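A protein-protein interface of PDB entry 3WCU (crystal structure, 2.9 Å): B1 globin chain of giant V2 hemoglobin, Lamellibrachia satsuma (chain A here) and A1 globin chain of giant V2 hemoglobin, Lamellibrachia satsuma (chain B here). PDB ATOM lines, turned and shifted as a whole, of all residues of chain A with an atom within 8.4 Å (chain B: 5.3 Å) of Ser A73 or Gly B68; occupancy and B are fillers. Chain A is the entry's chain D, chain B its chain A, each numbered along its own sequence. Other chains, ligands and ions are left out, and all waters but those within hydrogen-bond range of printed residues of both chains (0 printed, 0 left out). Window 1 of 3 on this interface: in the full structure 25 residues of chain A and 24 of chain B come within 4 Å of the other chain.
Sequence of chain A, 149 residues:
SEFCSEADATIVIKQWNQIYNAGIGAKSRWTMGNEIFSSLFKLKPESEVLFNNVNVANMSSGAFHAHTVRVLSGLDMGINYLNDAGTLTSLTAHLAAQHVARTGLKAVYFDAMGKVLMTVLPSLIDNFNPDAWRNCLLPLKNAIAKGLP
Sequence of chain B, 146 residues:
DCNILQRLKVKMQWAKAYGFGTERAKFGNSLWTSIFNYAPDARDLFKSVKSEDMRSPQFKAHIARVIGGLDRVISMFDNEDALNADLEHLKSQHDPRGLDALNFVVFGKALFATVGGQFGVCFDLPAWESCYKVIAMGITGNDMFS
The indole nitrogen (NE1) of Trp A16 sits at hydrogen-bond distance from the side-chain carboxylate (OD2) of Asp A76, at 2.8 Å. The side-chain hydroxyl of Tyr A20 sits at hydrogen-bond distance from the backbone NH of Ser A73, 3.4 Å away. O of Asp A76 is in hydrogen-bond range of ND2 of Asn A80.
Among the printed residues, pairs that only touch across the chains: Val A69 with Arg B72 (3.98 Å), Arg A70 with Arg B72 (3.5 Å), Ser A73 with Gly B68 (3.6 Å), Ser A73 with Arg B72 (3.4 Å), Met A77 with Arg B65 (3.9 Å) and Tyr A81 with Ala B64 (3.5 Å).
Ser A73 touches just these residues of chain B: Gly B68 (3.6 Å) and Arg B72 (3.4 Å). Of the printed residues of chain B, Val A69 touches Arg B72 (3.98 Å). Printed residues of chain A within 4 Å of Ala B64: Met A77 and Tyr A81. Printed residues of chain B within 4 Å of Asp A76: Asp B71 (3.3 Å). Arg A29 touches none of the printed residues of chain B. The nearest residue of chain A that does not touch Gly B68 is Met A77 (5.6 Å).
The side-chain carboxylate (OD1) of Asp A76 sits close to the side-chain carboxylate (OD2) of Asp B71. The backbone carbonyl oxygen (O) of Ala B64 lies close to the side-chain sulfur (SD) of Met A77 (3.5 Å).
Of the 20 printed residues of chain A, 6 touch a printed residue of chain B. Printed residues of chain A that touch a printed residue of chain B: Val A69, Arg A70, Ser A73, Asp A76, Met A77 and Tyr A81. Hydrophobic or aromatic side chains of chain A within 4 Å of the printed part of chain B: Val A69, Met A77 and Tyr A81. Among the printed residues, 8 pairs touch across the chains. Among the printed residues, no Asp or Glu carboxylate lies within 4 Å of a Lys or Arg side-chain nitrogen of the other chain.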
ATOM      1  N   TRP A  16     -14.167 -17.533  13.794  1.00  0.00           N
ATOM      2  CA  TRP A  16     -13.550 -18.252  12.691  1.00  0.00           C
ATOM      3  C   TRP A  16     -14.087 -19.660  12.571  1.00  0.00           C
ATOM      4  O   TRP A  16     -14.389 -20.110  11.470  1.00  0.00           O
ATOM      5  CB  TRP A  16     -12.037 -18.322  12.840  1.00  0.00           C
ATOM      6  CG  TRP A  16     -11.397 -19.079  11.723  1.00  0.00           C
ATOM      7  CD1 TRP A  16     -10.783 -20.302  11.797  1.00  0.00           C
ATOM      8  CD2 TRP A  16     -11.309 -18.669  10.351  1.00  0.00           C
ATOM      9  NE1 TRP A  16     -10.316 -20.676  10.555  1.00  0.00           N
ATOM     10  CE2 TRP A  16     -10.625 -19.693   9.651  1.00  0.00           C
ATOM     11  CE3 TRP A  16     -11.743 -17.538   9.641  1.00  0.00           C
ATOM     12  CZ2 TRP A  16     -10.367 -19.612   8.274  1.00  0.00           C
ATOM     13  CZ3 TRP A  16     -11.485 -17.462   8.273  1.00  0.00           C
ATOM     14  CH2 TRP A  16     -10.804 -18.493   7.608  1.00  0.00           C
ATOM     15  N   TYR A  20     -15.466 -21.661   9.258  1.00  0.00           N
ATOM     16  CA  TYR A  20     -14.400 -22.421   8.654  1.00  0.00           C
ATOM     17  C   TYR A  20     -14.067 -23.659   9.452  1.00  0.00           C
ATOM     18  O   TYR A  20     -13.567 -23.574  10.574  1.00  0.00           O
ATOM     19  CB  TYR A  20     -13.165 -21.542   8.480  1.00  0.00           C
ATOM     20  CG  TYR A  20     -12.130 -22.145   7.571  1.00  0.00           C
ATOM     21  CD1 TYR A  20     -11.374 -23.233   7.982  1.00  0.00           C
ATOM     22  CD2 TYR A  20     -11.920 -21.642   6.280  1.00  0.00           C
ATOM     23  CE1 TYR A  20     -10.431 -23.814   7.139  1.00  0.00           C
ATOM     24  CE2 TYR A  20     -10.982 -22.212   5.426  1.00  0.00           C
ATOM     25  CZ  TYR A  20     -10.239 -23.300   5.865  1.00  0.00           C
ATOM     26  OH  TYR A  20      -9.299 -23.885   5.047  1.00  0.00           O
ATOM     27  N   ARG A  29     -16.372 -23.424   0.634  1.00  0.00           N
ATOM     28  CA  ARG A  29     -14.932 -23.194   0.627  1.00  0.00           C
ATOM     29  C   ARG A  29     -14.603 -22.429  -0.637  1.00  0.00           C
ATOM     30  O   ARG A  29     -14.002 -21.353  -0.594  1.00  0.00           O
ATOM     31  CB  ARG A  29     -14.155 -24.498   0.608  1.00  0.00           C
ATOM     32  CG  ARG A  29     -14.880 -25.648   1.196  1.00  0.00           C
ATOM     33  CD  ARG A  29     -13.910 -26.762   1.475  1.00  0.00           C
ATOM     34  NE  ARG A  29     -13.056 -26.406   2.597  1.00  0.00           N
ATOM     35  CZ  ARG A  29     -13.480 -26.332   3.853  1.00  0.00           C
ATOM     36  NH1 ARG A  29     -14.745 -26.596   4.142  1.00  0.00           N
ATOM     37  NH2 ARG A  29     -12.644 -25.980   4.820  1.00  0.00           N
ATOM     38  N   ALA A  66      -7.564 -25.736  -4.739  1.00  0.00           N
ATOM     39  CA  ALA A  66      -6.693 -26.349  -3.744  1.00  0.00           C
ATOM     40  C   ALA A  66      -5.725 -25.324  -3.159  1.00  0.00           C
ATOM     41  O   ALA A  66      -5.415 -25.356  -1.969  1.00  0.00           O
ATOM     42  CB  ALA A  66      -5.919 -27.518  -4.352  1.00  0.00           C
ATOM     43  N   HIS A  67      -5.251 -24.404  -3.988  1.00  0.00           N
ATOM     44  CA  HIS A  67      -4.324 -23.391  -3.513  1.00  0.00           C
ATOM     45  C   HIS A  67      -4.962 -22.422  -2.527  1.00  0.00           C
ATOM     46  O   HIS A  67      -4.349 -22.064  -1.524  1.00  0.00           O
ATOM     47  CB  HIS A  67      -3.758 -22.594  -4.671  1.00  0.00           C
ATOM     48  CG  HIS A  67      -3.081 -21.335  -4.244  1.00  0.00           C
ATOM     49  ND1 HIS A  67      -1.809 -21.319  -3.716  1.00  0.00           N
ATOM     50  CD2 HIS A  67      -3.519 -20.053  -4.222  1.00  0.00           C
ATOM     51  CE1 HIS A  67      -1.492 -20.078  -3.391  1.00  0.00           C
ATOM     52  NE2 HIS A  67      -2.513 -19.291  -3.686  1.00  0.00           N
ATOM     53  N   THR A  68      -6.174 -21.968  -2.818  1.00  0.00           N
ATOM     54  CA  THR A  68      -6.820 -21.049  -1.901  1.00  0.00           C
ATOM     55  C   THR A  68      -7.096 -21.808  -0.619  1.00  0.00           C
ATOM     56  O   THR A  68      -7.030 -21.243   0.474  1.00  0.00           O
ATOM     57  CB  THR A  68      -8.154 -20.496  -2.445  1.00  0.00           C
ATOM     58  OG1 THR A  68      -9.119 -21.552  -2.551  1.00  0.00           O
ATOM     59  CG2 THR A  68      -7.942 -19.868  -3.797  1.00  0.00           C
ATOM     60  N   VAL A  69      -7.399 -23.096  -0.743  1.00  0.00           N
ATOM     61  CA  VAL A  69      -7.679 -23.881   0.444  1.00  0.00           C
ATOM     62  C   VAL A  69      -6.432 -24.036   1.296  1.00  0.00           C
ATOM     63  O   VAL A  69      -6.503 -23.880   2.515  1.00  0.00           O
ATOM     64  CB  VAL A  69      -8.314 -25.259   0.091  1.00  0.00           C
ATOM     65  CG1 VAL A  69      -8.024 -26.307   1.172  1.00  0.00           C
ATOM     66  CG2 VAL A  69      -9.836 -25.076  -0.035  1.00  0.00           C
ATOM     67  N   ARG A  70      -5.282 -24.306   0.694  1.00  0.00           N
ATOM     68  CA  ARG A  70      -4.110 -24.437   1.542  1.00  0.00           C
ATOM     69  C   ARG A  70      -3.609 -23.087   2.074  1.00  0.00           C
ATOM     70  O   ARG A  70      -2.808 -23.033   3.011  1.00  0.00           O
ATOM     71  CB  ARG A  70      -2.996 -25.240   0.851  1.00  0.00           C
ATOM     72  CG  ARG A  70      -2.706 -24.928  -0.587  1.00  0.00           C
ATOM     73  CD  ARG A  70      -1.626 -25.883  -1.062  1.00  0.00           C
ATOM     74  NE  ARG A  70      -2.027 -26.617  -2.257  1.00  0.00           N
ATOM     75  CZ  ARG A  70      -1.978 -26.136  -3.498  1.00  0.00           C
ATOM     76  NH1 ARG A  70      -1.538 -24.903  -3.727  1.00  0.00           N
ATOM     77  NH2 ARG A  70      -2.371 -26.897  -4.513  1.00  0.00           N
ATOM     78  N   VAL A  71      -4.092 -21.998   1.490  1.00  0.00           N
ATOM     79  CA  VAL A  71      -3.727 -20.675   1.984  1.00  0.00           C
ATOM     80  C   VAL A  71      -4.622 -20.480   3.205  1.00  0.00           C
ATOM     81  O   VAL A  71      -4.154 -20.210   4.312  1.00  0.00           O
ATOM     82  CB  VAL A  71      -4.068 -19.554   0.982  1.00  0.00           C
ATOM     83  CG1 VAL A  71      -3.840 -18.206   1.628  1.00  0.00           C
ATOM     84  CG2 VAL A  71      -3.234 -19.697  -0.271  1.00  0.00           C
ATOM     85  N   LEU A  72      -5.924 -20.622   2.983  1.00  0.00           N
ATOM     86  CA  LEU A  72      -6.893 -20.486   4.050  1.00  0.00           C
ATOM     87  C   LEU A  72      -6.676 -21.562   5.111  1.00  0.00           C
ATOM     88  O   LEU A  72      -7.029 -21.361   6.272  1.00  0.00           O
ATOM     89  CB  LEU A  72      -8.318 -20.565   3.492  1.00  0.00           C
ATOM     90  CG  LEU A  72      -8.796 -19.342   2.702  1.00  0.00           C
ATOM     91  CD1 LEU A  72     -10.281 -19.443   2.516  1.00  0.00           C
ATOM     92  CD2 LEU A  72      -8.489 -18.052   3.444  1.00  0.00           C
ATOM     93  N   SER A  73      -6.098 -22.698   4.721  1.00  0.00           N
ATOM     94  CA  SER A  73      -5.826 -23.773   5.680  1.00  0.00           C
ATOM     95  C   SER A  73      -4.680 -23.378   6.606  1.00  0.00           C
ATOM     96  O   SER A  73      -4.639 -23.807   7.757  1.00  0.00           O
ATOM     97  CB  SER A  73      -5.456 -25.078   4.969  1.00  0.00           C
ATOM     98  OG  SER A  73      -5.054 -26.071   5.904  1.00  0.00           O
ATOM     99  N   GLY A  74      -3.750 -22.576   6.076  1.00  0.00           N
ATOM    100  CA  GLY A  74      -2.609 -22.090   6.840  1.00  0.00           C
ATOM    101  C   GLY A  74      -3.064 -20.981   7.769  1.00  0.00           C
ATOM    102  O   GLY A  74      -2.555 -20.831   8.878  1.00  0.00           O
ATOM    103  N   LEU A  75      -4.029 -20.193   7.307  1.00  0.00           N
ATOM    104  CA  LEU A  75      -4.594 -19.128   8.117  1.00  0.00           C
ATOM    105  C   LEU A  75      -5.567 -19.753   9.127  1.00  0.00           C
ATOM    106  O   LEU A  75      -6.046 -19.084  10.035  1.00  0.00           O
ATOM    107  CB  LEU A  75      -5.341 -18.137   7.236  1.00  0.00           C
ATOM    108  CG  LEU A  75      -6.207 -17.156   8.025  1.00  0.00           C
ATOM    109  CD1 LEU A  75      -5.330 -16.158   8.775  1.00  0.00           C
ATOM    110  CD2 LEU A  75      -7.139 -16.443   7.079  1.00  0.00           C
ATOM    111  N   ASP A  76      -5.845 -21.045   8.953  1.00  0.00           N
ATOM    112  CA  ASP A  76      -6.740 -21.815   9.824  1.00  0.00           C
ATOM    113  C   ASP A  76      -5.938 -22.294  11.022  1.00  0.00           C
ATOM    114  O   ASP A  76      -6.429 -22.360  12.149  1.00  0.00           O
ATOM    115  CB  ASP A  76      -7.245 -23.050   9.080  1.00  0.00           C
ATOM    116  CG  ASP A  76      -8.326 -23.796   9.835  1.00  0.00           C
ATOM    117  OD1 ASP A  76      -8.505 -25.016   9.599  1.00  0.00           O
ATOM    118  OD2 ASP A  76      -9.015 -23.151  10.649  1.00  0.00           O
ATOM    119  N   MET A  77      -4.694 -22.649  10.739  1.00  0.00           N
ATOM    120  CA  MET A  77      -3.758 -23.161  11.718  1.00  0.00           C
ATOM    121  C   MET A  77      -3.221 -22.056  12.618  1.00  0.00           C
ATOM    122  O   MET A  77      -2.864 -22.305  13.772  1.00  0.00           O
ATOM    123  CB  MET A  77      -2.627 -23.850  10.969  1.00  0.00           C
ATOM    124  CG  MET A  77      -1.394 -24.133  11.766  1.00  0.00           C
ATOM    125  SD  MET A  77      -0.114 -24.754  10.654  1.00  0.00           S
ATOM    126  CE  MET A  77       0.363 -23.256   9.802  1.00  0.00           C
ATOM    127  N   GLY A  78      -3.173 -20.838  12.089  1.00  0.00           N
ATOM    128  CA  GLY A  78      -2.682 -19.717  12.866  1.00  0.00           C
ATOM    129  C   GLY A  78      -3.724 -19.239  13.855  1.00  0.00           C
ATOM    130  O   GLY A  78      -3.450 -19.067  15.038  1.00  0.00           O
ATOM    131  N   ILE A  79      -4.929 -19.012  13.363  1.00  0.00           N
ATOM    132  CA  ILE A  79      -6.020 -18.565  14.206  1.00  0.00           C
ATOM    133  C   ILE A  79      -6.264 -19.568  15.340  1.00  0.00           C
ATOM    134  O   ILE A  79      -6.512 -19.167  16.469  1.00  0.00           O
ATOM    135  CB  ILE A  79      -7.314 -18.400  13.357  1.00  0.00           C
ATOM    136  CG1 ILE A  79      -7.245 -17.093  12.562  1.00  0.00           C
ATOM    137  CG2 ILE A  79      -8.541 -18.459  14.232  1.00  0.00           C
ATOM    138  CD1 ILE A  79      -8.520 -16.745  11.778  1.00  0.00           C
ATOM    139  N   ASN A  80      -6.176 -20.861  15.029  1.00  0.00           N
ATOM    140  CA  ASN A  80      -6.414 -21.935  15.992  1.00  0.00           C
ATOM    141  C   ASN A  80      -5.230 -22.223  16.918  1.00  0.00           C
ATOM    142  O   ASN A  80      -5.304 -23.087  17.805  1.00  0.00           O
ATOM    143  CB  ASN A  80      -6.788 -23.227  15.256  1.00  0.00           C
ATOM    144  CG  ASN A  80      -8.261 -23.315  14.920  1.00  0.00           C
ATOM    145  OD1 ASN A  80      -9.109 -23.253  15.803  1.00  0.00           O
ATOM    146  ND2 ASN A  80      -8.573 -23.473  13.636  1.00  0.00           N
ATOM    147  N   TYR A  81      -4.131 -21.514  16.705  1.00  0.00           N
ATOM    148  CA  TYR A  81      -2.950 -21.682  17.539  1.00  0.00           C
ATOM    149  C   TYR A  81      -2.563 -20.361  18.178  1.00  0.00           C
ATOM    150  O   TYR A  81      -1.451 -20.203  18.669  1.00  0.00           O
ATOM    151  CB  TYR A  81      -1.797 -22.199  16.707  1.00  0.00           C
ATOM    152  CG  TYR A  81      -1.690 -23.691  16.714  1.00  0.00           C
ATOM    153  CD1 TYR A  81      -0.722 -24.330  17.494  1.00  0.00           C
ATOM    154  CD2 TYR A  81      -2.535 -24.474  15.932  1.00  0.00           C
ATOM    155  CE1 TYR A  81      -0.590 -25.706  17.491  1.00  0.00           C
ATOM    156  CE2 TYR A  81      -2.409 -25.872  15.922  1.00  0.00           C
ATOM    157  CZ  TYR A  81      -1.430 -26.476  16.704  1.00  0.00           C
ATOM    158  OH  TYR A  81      -1.267 -27.847  16.690  1.00  0.00           O
ATOM    159  N   LEU A  95       6.357 -19.930   7.616  1.00  0.00           N
ATOM    160  CA  LEU A  95       5.573 -19.359   6.512  1.00  0.00           C
ATOM    161  C   LEU A  95       6.242 -18.149   5.852  1.00  0.00           C
ATOM    162  O   LEU A  95       5.950 -17.817   4.702  1.00  0.00           O
ATOM    163  CB  LEU A  95       4.170 -18.956   6.992  1.00  0.00           C
ATOM    164  CG  LEU A  95       3.156 -20.097   7.100  1.00  0.00           C
ATOM    165  CD1 LEU A  95       1.986 -19.652   7.943  1.00  0.00           C
ATOM    166  CD2 LEU A  95       2.693 -20.525   5.721  1.00  0.00           C
ATOM    167  N   TYR B  18     -11.521 -33.442  15.777  1.00  0.00           N
ATOM    168  CA  TYR B  18     -10.387 -32.518  15.694  1.00  0.00           C
ATOM    169  C   TYR B  18     -10.558 -31.265  16.555  1.00  0.00           C
ATOM    170  O   TYR B  18      -9.579 -30.730  17.077  1.00  0.00           O
ATOM    171  CB  TYR B  18     -10.109 -32.115  14.230  1.00  0.00           C
ATOM    172  CG  TYR B  18      -8.737 -31.498  14.044  1.00  0.00           C
ATOM    173  CD1 TYR B  18      -7.623 -32.033  14.708  1.00  0.00           C
ATOM    174  CD2 TYR B  18      -8.541 -30.370  13.236  1.00  0.00           C
ATOM    175  CE1 TYR B  18      -6.348 -31.458  14.581  1.00  0.00           C
ATOM    176  CE2 TYR B  18      -7.256 -29.786  13.097  1.00  0.00           C
ATOM    177  CZ  TYR B  18      -6.163 -30.338  13.777  1.00  0.00           C
ATOM    178  OH  TYR B  18      -4.895 -29.790  13.662  1.00  0.00           O
ATOM    179  N   ILE B  63       3.489 -30.783  13.893  1.00  0.00           N
ATOM    180  CA  ILE B  63       2.211 -31.437  14.104  1.00  0.00           C
ATOM    181  C   ILE B  63       1.129 -30.520  13.557  1.00  0.00           C
ATOM    182  O   ILE B  63       0.219 -30.966  12.867  1.00  0.00           O
ATOM    183  CB  ILE B  63       1.923 -31.673  15.599  1.00  0.00           C
ATOM    184  CG1 ILE B  63       3.028 -32.528  16.221  1.00  0.00           C
ATOM    185  CG2 ILE B  63       0.572 -32.356  15.756  1.00  0.00           C
ATOM    186  CD1 ILE B  63       2.744 -32.964  17.644  1.00  0.00           C
ATOM    187  N   ALA B  64       1.244 -29.233  13.864  1.00  0.00           N
ATOM    188  CA  ALA B  64       0.272 -28.252  13.415  1.00  0.00           C
ATOM    189  C   ALA B  64       0.194 -28.217  11.903  1.00  0.00           C
ATOM    190  O   ALA B  64      -0.888 -28.049  11.339  1.00  0.00           O
ATOM    191  CB  ALA B  64       0.629 -26.875  13.944  1.00  0.00           C
ATOM    192  N   ARG B  65       1.344 -28.370  11.252  1.00  0.00           N
ATOM    193  CA  ARG B  65       1.407 -28.353   9.797  1.00  0.00           C
ATOM    194  C   ARG B  65       0.799 -29.584   9.132  1.00  0.00           C
ATOM    195  O   ARG B  65       0.039 -29.461   8.177  1.00  0.00           O
ATOM    196  CB  ARG B  65       2.859 -28.186   9.319  1.00  0.00           C
ATOM    197  CG  ARG B  65       3.306 -26.732   9.117  1.00  0.00           C
ATOM    198  CD  ARG B  65       4.559 -26.660   8.263  1.00  0.00           C
ATOM    199  NE  ARG B  65       5.687 -27.272   8.948  1.00  0.00           N
ATOM    200  CZ  ARG B  65       6.301 -26.723   9.990  1.00  0.00           C
ATOM    201  NH1 ARG B  65       5.887 -25.549  10.447  1.00  0.00           N
ATOM    202  NH2 ARG B  65       7.313 -27.351  10.575  1.00  0.00           N
ATOM    203  N   VAL B  66       1.128 -30.763   9.645  1.00  0.00           N
ATOM    204  CA  VAL B  66       0.648 -32.024   9.083  1.00  0.00           C
ATOM    205  C   VAL B  66      -0.819 -32.345   9.266  1.00  0.00           C
ATOM    206  O   VAL B  66      -1.551 -32.475   8.292  1.00  0.00           O
ATOM    207  CB  VAL B  66       1.444 -33.222   9.627  1.00  0.00           C
ATOM    208  CG1 VAL B  66       0.818 -34.526   9.142  1.00  0.00           C
ATOM    209  CG2 VAL B  66       2.891 -33.119   9.170  1.00  0.00           C
ATOM    210  N   ILE B  67      -1.258 -32.520  10.502  1.00  0.00           N
ATOM    211  CA  ILE B  67      -2.655 -32.831  10.692  1.00  0.00           C
ATOM    212  C   ILE B  67      -3.445 -31.579  10.305  1.00  0.00           C
ATOM    213  O   ILE B  67      -4.663 -31.613  10.115  1.00  0.00           O
ATOM    214  CB  ILE B  67      -2.912 -33.265  12.120  1.00  0.00           C
ATOM    215  CG1 ILE B  67      -2.973 -32.056  13.030  1.00  0.00           C
ATOM    216  CG2 ILE B  67      -1.793 -34.204  12.560  1.00  0.00           C
ATOM    217  CD1 ILE B  67      -3.202 -32.413  14.469  1.00  0.00           C
ATOM    218  N   GLY B  68      -2.728 -30.467  10.172  1.00  0.00           N
ATOM    219  CA  GLY B  68      -3.361 -29.240   9.744  1.00  0.00           C
ATOM    220  C   GLY B  68      -3.652 -29.525   8.287  1.00  0.00           C
ATOM    221  O   GLY B  68      -4.684 -29.134   7.741  1.00  0.00           O
ATOM    222  N   GLY B  69      -2.725 -30.228   7.646  1.00  0.00           N
ATOM    223  CA  GLY B  69      -2.908 -30.596   6.256  1.00  0.00           C
ATOM    224  C   GLY B  69      -3.998 -31.649   6.177  1.00  0.00           C
ATOM    225  O   GLY B  69      -4.931 -31.536   5.383  1.00  0.00           O
ATOM    226  N   LEU B  70      -3.875 -32.682   7.003  1.00  0.00           N
ATOM    227  CA  LEU B  70      -4.870 -33.731   7.033  1.00  0.00           C
ATOM    228  C   LEU B  70      -6.236 -33.068   7.054  1.00  0.00           C
ATOM    229  O   LEU B  70      -7.133 -33.464   6.314  1.00  0.00           O
ATOM    230  CB  LEU B  70      -4.717 -34.590   8.280  1.00  0.00           C
ATOM    231  CG  LEU B  70      -5.080 -36.058   8.072  1.00  0.00           C
ATOM    232  CD1 LEU B  70      -5.512 -36.668   9.392  1.00  0.00           C
ATOM    233  CD2 LEU B  70      -6.191 -36.172   7.052  1.00  0.00           C
ATOM    234  N   ASP B  71      -6.392 -32.048   7.897  1.00  0.00           N
ATOM    235  CA  ASP B  71      -7.661 -31.338   7.984  1.00  0.00           C
ATOM    236  C   ASP B  71      -8.079 -30.807   6.611  1.00  0.00           C
ATOM    237  O   ASP B  71      -9.169 -31.108   6.146  1.00  0.00           O
ATOM    238  CB  ASP B  71      -7.571 -30.169   8.980  1.00  0.00           C
ATOM    239  CG  ASP B  71      -8.912 -29.416   9.155  1.00  0.00           C
ATOM    240  OD1 ASP B  71      -9.885 -30.035   9.661  1.00  0.00           O
ATOM    241  OD2 ASP B  71      -8.981 -28.206   8.797  1.00  0.00           O
ATOM    242  N   ARG B  72      -7.224 -30.030   5.949  1.00  0.00           N
ATOM    243  CA  ARG B  72      -7.605 -29.487   4.651  1.00  0.00           C
ATOM    244  C   ARG B  72      -7.920 -30.576   3.641  1.00  0.00           C
ATOM    245  O   ARG B  72      -8.943 -30.516   2.960  1.00  0.00           O
ATOM    246  CB  ARG B  72      -6.527 -28.550   4.096  1.00  0.00           C
ATOM    247  CG  ARG B  72      -5.404 -29.197   3.314  1.00  0.00           C
ATOM    248  CD  ARG B  72      -4.669 -28.115   2.554  1.00  0.00           C
ATOM    249  NE  ARG B  72      -3.492 -28.595   1.839  1.00  0.00           N
ATOM    250  CZ  ARG B  72      -2.337 -28.913   2.414  1.00  0.00           C
ATOM    251  NH1 ARG B  72      -2.196 -28.809   3.728  1.00  0.00           N
ATOM    252  NH2 ARG B  72      -1.314 -29.312   1.667  1.00  0.00           N
